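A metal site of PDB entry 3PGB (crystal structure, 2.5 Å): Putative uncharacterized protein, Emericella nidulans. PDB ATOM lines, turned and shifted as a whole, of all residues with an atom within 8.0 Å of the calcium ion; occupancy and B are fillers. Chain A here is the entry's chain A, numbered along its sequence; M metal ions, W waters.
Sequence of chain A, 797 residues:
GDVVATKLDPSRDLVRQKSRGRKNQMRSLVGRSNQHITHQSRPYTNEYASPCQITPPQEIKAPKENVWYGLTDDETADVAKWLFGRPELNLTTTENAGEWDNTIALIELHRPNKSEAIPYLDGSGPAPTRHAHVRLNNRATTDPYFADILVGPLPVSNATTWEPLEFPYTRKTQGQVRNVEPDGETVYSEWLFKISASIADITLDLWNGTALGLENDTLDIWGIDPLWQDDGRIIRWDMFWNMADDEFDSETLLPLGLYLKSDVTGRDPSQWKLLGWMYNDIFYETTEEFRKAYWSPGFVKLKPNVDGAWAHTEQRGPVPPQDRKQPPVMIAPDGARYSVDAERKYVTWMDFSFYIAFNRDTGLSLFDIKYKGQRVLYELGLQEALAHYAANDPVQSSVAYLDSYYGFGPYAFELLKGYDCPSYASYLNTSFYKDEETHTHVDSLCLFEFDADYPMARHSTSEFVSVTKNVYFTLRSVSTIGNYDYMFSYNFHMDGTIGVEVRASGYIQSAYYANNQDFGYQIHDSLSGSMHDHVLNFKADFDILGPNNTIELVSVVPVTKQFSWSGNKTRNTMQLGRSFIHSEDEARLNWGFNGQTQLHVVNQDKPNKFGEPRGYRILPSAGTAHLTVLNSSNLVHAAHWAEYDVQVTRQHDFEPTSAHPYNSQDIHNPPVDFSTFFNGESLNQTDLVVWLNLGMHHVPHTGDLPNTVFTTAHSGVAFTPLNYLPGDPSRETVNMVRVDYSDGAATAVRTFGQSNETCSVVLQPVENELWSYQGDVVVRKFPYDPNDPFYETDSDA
NZ of Lys 114 is in salt-bridge range of OD2 of Asp 543 (2.7 Å).
The backbone NH (N) of Asp 543 is in hydrogen-bond range of the backbone carbonyl oxygen (O) of Val 376, 3.0 Å away.
The side-chain carboxylate (OD2) of Asp 687 lies within salt-bridge range of the side-chain amino group (NZ) of Lys 114, 2.9 Å away.
The backbone carbonyl oxygen of Asp 687 lies within hydrogen-bond range of the backbone NH of Gln 651 (2.8 Å).
OD2 of Asp 541 is in salt-bridge range of NZ of Lys 114 (2.8 Å).
O of Asp 541 sits at hydrogen-bond distance from N of Tyr 378 (2.9 Å).
The backbone NH of Asp 541 sits at hydrogen-bond distance from the backbone carbonyl oxygen of Glu 379, at 2.9 Å.
The backbone carbonyl oxygen (O) of Phe 542 lies close to the side-chain amide oxygen (OD1) of Asn 549 (3.2 Å).
Lys 114 touches the calcium ion.
Of the 23 residues printed, 6 come within 4 Å of the calcium ion.
The nearest printed residue that does not touch the calcium ion is Pro 547 (4.4 Å).
The calcium ion is bound by OD1 of Asp 543, 2.3 Å away.
The side-chain carboxylate (OD1) of Asp 687 is bound to the calcium ion (2.3 Å).
OD1 of Asp 541 is bound to the calcium ion.
The calcium ion is bound by O of Leu 688.
O of Phe 542 is bound to the calcium ion, 2.5 Å away.
Water W1 binds the calcium ion (2.5 Å).
The calcium ion has six donor atoms within binding distance.
Water W1 lies within hydrogen-bond range of OD1 of Asn 549, O of Pro 547 and N of Leu 688.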
ATOM      1  N   LYS A 114      -2.891  19.395  29.220  1.00  0.00           N
ATOM      2  CA  LYS A 114      -3.991  18.795  29.985  1.00  0.00           C
ATOM      3  C   LYS A 114      -3.970  17.271  29.888  1.00  0.00           C
ATOM      4  O   LYS A 114      -4.281  16.576  30.853  1.00  0.00           O
ATOM      5  CB  LYS A 114      -5.328  19.346  29.497  1.00  0.00           C
ATOM      6  CG  LYS A 114      -6.542  18.930  30.315  1.00  0.00           C
ATOM      7  CD  LYS A 114      -7.819  19.487  29.700  1.00  0.00           C
ATOM      8  CE  LYS A 114      -9.059  18.948  30.388  1.00  0.00           C
ATOM      9  NZ  LYS A 114     -10.267  19.747  30.039  1.00  0.00           N
ATOM     10  N   VAL A 376     -15.157  20.496  38.514  1.00  0.00           N
ATOM     11  CA  VAL A 376     -16.084  21.268  37.664  1.00  0.00           C
ATOM     12  C   VAL A 376     -15.329  22.121  36.653  1.00  0.00           C
ATOM     13  O   VAL A 376     -15.836  22.360  35.563  1.00  0.00           O
ATOM     14  CB  VAL A 376     -17.056  22.142  38.505  1.00  0.00           C
ATOM     15  CG1 VAL A 376     -17.373  21.469  39.833  1.00  0.00           C
ATOM     16  CG2 VAL A 376     -16.502  23.534  38.707  1.00  0.00           C
ATOM     17  N   LEU A 377     -14.121  22.561  37.002  1.00  0.00           N
ATOM     18  CA  LEU A 377     -13.262  23.330  36.102  1.00  0.00           C
ATOM     19  C   LEU A 377     -11.808  22.868  36.201  1.00  0.00           C
ATOM     20  O   LEU A 377     -11.220  22.893  37.278  1.00  0.00           O
ATOM     21  CB  LEU A 377     -13.337  24.820  36.439  1.00  0.00           C
ATOM     22  CG  LEU A 377     -14.657  25.566  36.160  1.00  0.00           C
ATOM     23  CD1 LEU A 377     -14.985  26.541  37.287  1.00  0.00           C
ATOM     24  CD2 LEU A 377     -14.602  26.286  34.830  1.00  0.00           C
ATOM     25  N   TYR A 378     -11.243  22.436  35.086  1.00  0.00           N
ATOM     26  CA  TYR A 378      -9.824  22.097  35.030  1.00  0.00           C
ATOM     27  C   TYR A 378      -8.974  23.357  35.169  1.00  0.00           C
ATOM     28  O   TYR A 378      -7.916  23.335  35.785  1.00  0.00           O
ATOM     29  CB  TYR A 378      -9.458  21.360  33.725  1.00  0.00           C
ATOM     30  CG  TYR A 378      -7.960  21.184  33.528  1.00  0.00           C
ATOM     31  CD1 TYR A 378      -7.270  20.189  34.202  1.00  0.00           C
ATOM     32  CD2 TYR A 378      -7.248  22.030  32.691  1.00  0.00           C
ATOM     33  CE1 TYR A 378      -5.901  20.035  34.040  1.00  0.00           C
ATOM     34  CE2 TYR A 378      -5.872  21.881  32.526  1.00  0.00           C
ATOM     35  CZ  TYR A 378      -5.214  20.881  33.201  1.00  0.00           C
ATOM     36  OH  TYR A 378      -3.850  20.737  33.041  1.00  0.00           O
ATOM     37  N   GLU A 379      -9.450  24.457  34.591  1.00  0.00           N
ATOM     38  CA  GLU A 379      -8.698  25.699  34.520  1.00  0.00           C
ATOM     39  C   GLU A 379      -9.629  26.912  34.441  1.00  0.00           C
ATOM     40  O   GLU A 379     -10.606  26.895  33.691  1.00  0.00           O
ATOM     41  CB  GLU A 379      -7.755  25.680  33.311  1.00  0.00           C
ATOM     42  CG  GLU A 379      -6.875  26.935  33.185  1.00  0.00           C
ATOM     43  CD  GLU A 379      -6.060  26.972  31.895  1.00  0.00           C
ATOM     44  OE1 GLU A 379      -5.205  27.878  31.782  1.00  0.00           O
ATOM     45  OE2 GLU A 379      -6.278  26.128  30.993  1.00  0.00           O
ATOM     46  N   ALA A 540     -12.518  29.440  30.864  1.00  0.00           N
ATOM     47  CA  ALA A 540     -13.270  28.593  31.789  1.00  0.00           C
ATOM     48  C   ALA A 540     -13.387  27.179  31.212  1.00  0.00           C
ATOM     49  O   ALA A 540     -14.308  26.890  30.448  1.00  0.00           O
ATOM     50  CB  ALA A 540     -14.639  29.183  32.064  1.00  0.00           C
ATOM     51  N   ASP A 541     -12.450  26.312  31.559  1.00  0.00           N
ATOM     52  CA  ASP A 541     -12.438  24.945  31.055  1.00  0.00           C
ATOM     53  C   ASP A 541     -13.293  24.046  31.941  1.00  0.00           C
ATOM     54  O   ASP A 541     -12.773  23.235  32.710  1.00  0.00           O
ATOM     55  CB  ASP A 541     -11.003  24.405  30.980  1.00  0.00           C
ATOM     56  CG  ASP A 541     -10.913  23.055  30.279  1.00  0.00           C
ATOM     57  OD1 ASP A 541     -11.933  22.548  29.789  1.00  0.00           O
ATOM     58  OD2 ASP A 541      -9.805  22.490  30.243  1.00  0.00           O
ATOM     59  N   PHE A 542     -14.614  24.181  31.832  1.00  0.00           N
ATOM     60  CA  PHE A 542     -15.526  23.316  32.569  1.00  0.00           C
ATOM     61  C   PHE A 542     -15.386  21.881  32.093  1.00  0.00           C
ATOM     62  O   PHE A 542     -15.426  21.630  30.895  1.00  0.00           O
ATOM     63  CB  PHE A 542     -16.987  23.739  32.355  1.00  0.00           C
ATOM     64  CG  PHE A 542     -17.321  25.086  32.887  1.00  0.00           C
ATOM     65  CD1 PHE A 542     -17.768  25.237  34.199  1.00  0.00           C
ATOM     66  CD2 PHE A 542     -17.197  26.209  32.100  1.00  0.00           C
ATOM     67  CE1 PHE A 542     -18.067  26.472  34.696  1.00  0.00           C
ATOM     68  CE2 PHE A 542     -17.501  27.444  32.587  1.00  0.00           C
ATOM     69  CZ  PHE A 542     -17.933  27.582  33.884  1.00  0.00           C
ATOM     70  N   ASP A 543     -15.205  20.949  33.031  1.00  0.00           N
ATOM     71  CA  ASP A 543     -15.280  19.518  32.725  1.00  0.00           C
ATOM     72  C   ASP A 543     -16.362  18.917  33.611  1.00  0.00           C
ATOM     73  O   ASP A 543     -16.075  18.207  34.579  1.00  0.00           O
ATOM     74  CB  ASP A 543     -13.937  18.831  32.987  1.00  0.00           C
ATOM     75  CG  ASP A 543     -12.866  19.207  31.963  1.00  0.00           C
ATOM     76  OD1 ASP A 543     -13.185  19.815  30.920  1.00  0.00           O
ATOM     77  OD2 ASP A 543     -11.691  18.880  32.215  1.00  0.00           O
ATOM     78  N   ILE A 544     -17.624  19.188  33.261  1.00  0.00           N
ATOM     79  CA  ILE A 544     -18.738  18.820  34.131  1.00  0.00           C
ATOM     80  C   ILE A 544     -18.909  17.296  34.164  1.00  0.00           C
ATOM     81  O   ILE A 544     -19.272  16.682  33.157  1.00  0.00           O
ATOM     82  CB  ILE A 544     -20.064  19.500  33.704  1.00  0.00           C
ATOM     83  CG1 ILE A 544     -19.913  21.025  33.614  1.00  0.00           C
ATOM     84  CG2 ILE A 544     -21.186  19.143  34.672  1.00  0.00           C
ATOM     85  CD1 ILE A 544     -19.375  21.673  34.878  1.00  0.00           C
ATOM     86  N   GLY A 546     -16.760  15.040  34.107  1.00  0.00           N
ATOM     87  CA  GLY A 546     -15.937  14.506  33.037  1.00  0.00           C
ATOM     88  C   GLY A 546     -15.761  15.513  31.913  1.00  0.00           C
ATOM     89  O   GLY A 546     -16.451  16.531  31.864  1.00  0.00           O
ATOM     90  N   PRO A 547     -14.828  15.240  30.979  1.00  0.00           N
ATOM     91  CA  PRO A 547     -14.530  16.183  29.907  1.00  0.00           C
ATOM     92  C   PRO A 547     -15.631  16.297  28.852  1.00  0.00           C
ATOM     93  O   PRO A 547     -15.813  17.376  28.277  1.00  0.00           O
ATOM     94  CB  PRO A 547     -13.239  15.625  29.310  1.00  0.00           C
ATOM     95  CG  PRO A 547     -13.290  14.159  29.577  1.00  0.00           C
ATOM     96  CD  PRO A 547     -14.084  13.978  30.847  1.00  0.00           C
ATOM     97  N   ASN A 548     -16.366  15.212  28.592  1.00  0.00           N
ATOM     98  CA  ASN A 548     -17.390  15.218  27.530  1.00  0.00           C
ATOM     99  C   ASN A 548     -18.643  16.034  27.906  1.00  0.00           C
ATOM    100  O   ASN A 548     -19.534  15.523  28.589  1.00  0.00           O
ATOM    101  CB  ASN A 548     -17.785  13.778  27.134  1.00  0.00           C
ATOM    102  CG  ASN A 548     -16.628  12.990  26.484  1.00  0.00           C
ATOM    103  OD1 ASN A 548     -15.671  13.570  25.960  1.00  0.00           O
ATOM    104  ND2 ASN A 548     -16.722  11.657  26.515  1.00  0.00           N
ATOM    105  N   ASN A 549     -18.683  17.298  27.476  1.00  0.00           N
ATOM    106  CA  ASN A 549     -19.794  18.225  27.784  1.00  0.00           C
ATOM    107  C   ASN A 549     -20.493  18.803  26.544  1.00  0.00           C
ATOM    108  O   ASN A 549     -20.018  18.654  25.423  1.00  0.00           O
ATOM    109  CB  ASN A 549     -19.267  19.389  28.627  1.00  0.00           C
ATOM    110  CG  ASN A 549     -18.710  18.949  29.971  1.00  0.00           C
ATOM    111  OD1 ASN A 549     -17.967  19.703  30.615  1.00  0.00           O
ATOM    112  ND2 ASN A 549     -19.054  17.743  30.399  1.00  0.00           N
ATOM    113  N   VAL A 601     -23.558  24.833  30.788  1.00  0.00           N
ATOM    114  CA  VAL A 601     -22.526  23.885  30.390  1.00  0.00           C
ATOM    115  C   VAL A 601     -22.902  22.569  31.039  1.00  0.00           C
ATOM    116  O   VAL A 601     -22.822  22.435  32.248  1.00  0.00           O
ATOM    117  CB  VAL A 601     -21.114  24.322  30.848  1.00  0.00           C
ATOM    118  CG1 VAL A 601     -20.067  23.317  30.371  1.00  0.00           C
ATOM    119  CG2 VAL A 601     -20.787  25.695  30.314  1.00  0.00           C
ATOM    120  N   THR A 649     -15.142  26.807  22.243  1.00  0.00           N
ATOM    121  CA  THR A 649     -14.297  26.056  21.321  1.00  0.00           C
ATOM    122  C   THR A 649     -13.978  24.712  21.928  1.00  0.00           C
ATOM    123  O   THR A 649     -14.067  24.521  23.142  1.00  0.00           O
ATOM    124  CB  THR A 649     -12.952  26.758  21.055  1.00  0.00           C
ATOM    125  OG1 THR A 649     -12.186  26.797  22.261  1.00  0.00           O
ATOM    126  CG2 THR A 649     -13.159  28.163  20.526  1.00  0.00           C
ATOM    127  N   ARG A 650     -13.591  23.772  21.067  1.00  0.00           N
ATOM    128  CA  ARG A 650     -13.173  22.464  21.535  1.00  0.00           C
ATOM    129  C   ARG A 650     -11.784  22.577  22.122  1.00  0.00           C
ATOM    130  O   ARG A 650     -10.935  23.288  21.584  1.00  0.00           O
ATOM    131  CB  ARG A 650     -13.186  21.442  20.410  1.00  0.00           C
ATOM    132  CG  ARG A 650     -12.853  20.059  20.894  1.00  0.00           C
ATOM    133  CD  ARG A 650     -13.149  19.012  19.868  1.00  0.00           C
ATOM    134  NE  ARG A 650     -13.018  17.688  20.435  1.00  0.00           N
ATOM    135  CZ  ARG A 650     -13.093  16.562  19.732  1.00  0.00           C
ATOM    136  NH1 ARG A 650     -13.312  16.596  18.411  1.00  0.00           N
ATOM    137  NH2 ARG A 650     -12.962  15.385  20.354  1.00  0.00           N
ATOM    138  N   GLN A 651     -11.567  21.875  23.242  1.00  0.00           N
ATOM    139  CA  GLN A 651     -10.286  21.930  23.940  1.00  0.00           C
ATOM    140  C   GLN A 651      -9.177  21.274  23.108  1.00  0.00           C
ATOM    141  O   GLN A 651      -9.371  20.219  22.511  1.00  0.00           O
ATOM    142  CB  GLN A 651     -10.393  21.245  25.311  1.00  0.00           C
ATOM    143  CG  GLN A 651      -9.257  21.583  26.298  1.00  0.00           C
ATOM    144  CD  GLN A 651      -7.958  20.810  26.054  1.00  0.00           C
ATOM    145  OE1 GLN A 651      -7.960  19.731  25.464  1.00  0.00           O
ATOM    146  NE2 GLN A 651      -6.844  21.374  26.523  1.00  0.00           N
ATOM    147  N   THR A 686     -18.192  16.698  23.662  1.00  0.00           N
ATOM    148  CA  THR A 686     -16.735  16.650  23.577  1.00  0.00           C
ATOM    149  C   THR A 686     -16.197  17.578  24.644  1.00  0.00           C
ATOM    150  O   THR A 686     -16.981  18.215  25.363  1.00  0.00           O
ATOM    151  CB  THR A 686     -16.215  17.102  22.196  1.00  0.00           C
ATOM    152  OG1 THR A 686     -16.349  18.514  22.065  1.00  0.00           O
ATOM    153  CG2 THR A 686     -16.983  16.401  21.074  1.00  0.00           C
ATOM    154  N   ASP A 687     -14.870  17.658  24.755  1.00  0.00           N
ATOM    155  CA  ASP A 687     -14.225  18.556  25.711  1.00  0.00           C
ATOM    156  C   ASP A 687     -14.255  19.977  25.174  1.00  0.00           C
ATOM    157  O   ASP A 687     -13.617  20.294  24.173  1.00  0.00           O
ATOM    158  CB  ASP A 687     -12.773  18.109  25.970  1.00  0.00           C
ATOM    159  CG  ASP A 687     -12.101  18.861  27.126  1.00  0.00           C
ATOM    160  OD1 ASP A 687     -12.603  19.942  27.520  1.00  0.00           O
ATOM    161  OD2 ASP A 687     -11.072  18.374  27.638  1.00  0.00           O
ATOM    162  N   LEU A 688     -15.023  20.842  25.838  1.00  0.00           N
ATOM    163  CA  LEU A 688     -15.152  22.223  25.398  1.00  0.00           C
ATOM    164  C   LEU A 688     -14.500  23.196  26.384  1.00  0.00           C
ATOM    165  O   LEU A 688     -14.276  22.847  27.550  1.00  0.00           O
ATOM    166  CB  LEU A 688     -16.627  22.589  25.156  1.00  0.00           C
ATOM    167  CG  LEU A 688     -17.668  22.208  26.222  1.00  0.00           C
ATOM    168  CD1 LEU A 688     -17.519  23.084  27.456  1.00  0.00           C
ATOM    169  CD2 LEU A 688     -19.086  22.292  25.647  1.00  0.00           C
ATOM    170  N   VAL A 689     -14.180  24.381  25.890  1.00  0.00           N
ATOM    171  CA  VAL A 689     -13.681  25.469  26.710  1.00  0.00           C
ATOM    172  C   VAL A 689     -14.604  26.658  26.480  1.00  0.00           C
ATOM    173  O   VAL A 689     -14.867  27.029  25.339  1.00  0.00           O
ATOM    174  CB  VAL A 689     -12.254  25.864  26.314  1.00  0.00           C
ATOM    175  CG1 VAL A 689     -11.755  27.010  27.188  1.00  0.00           C
ATOM    176  CG2 VAL A 689     -11.333  24.687  26.418  1.00  0.00           C
ATOM    177  N   VAL A 690     -15.095  27.242  27.562  1.00  0.00           N
ATOM    178  CA  VAL A 690     -15.899  28.458  27.481  1.00  0.00           C
ATOM    179  C   VAL A 690     -14.987  29.649  27.735  1.00  0.00           C
ATOM    180  O   VAL A 690     -14.362  29.741  28.779  1.00  0.00           O
ATOM    181  CB  VAL A 690     -17.051  28.428  28.486  1.00  0.00           C
ATOM    182  CG1 VAL A 690     -17.918  29.673  28.333  1.00  0.00           C
ATOM    183  CG2 VAL A 690     -17.874  27.168  28.285  1.00  0.00           C
HETATM  184 CA    CA M   1     -13.747  21.151  29.169  1.00  0.00          CA
HETATM  185  O   HOH W   1     -16.027  20.172  28.686  1.00  0.00           O
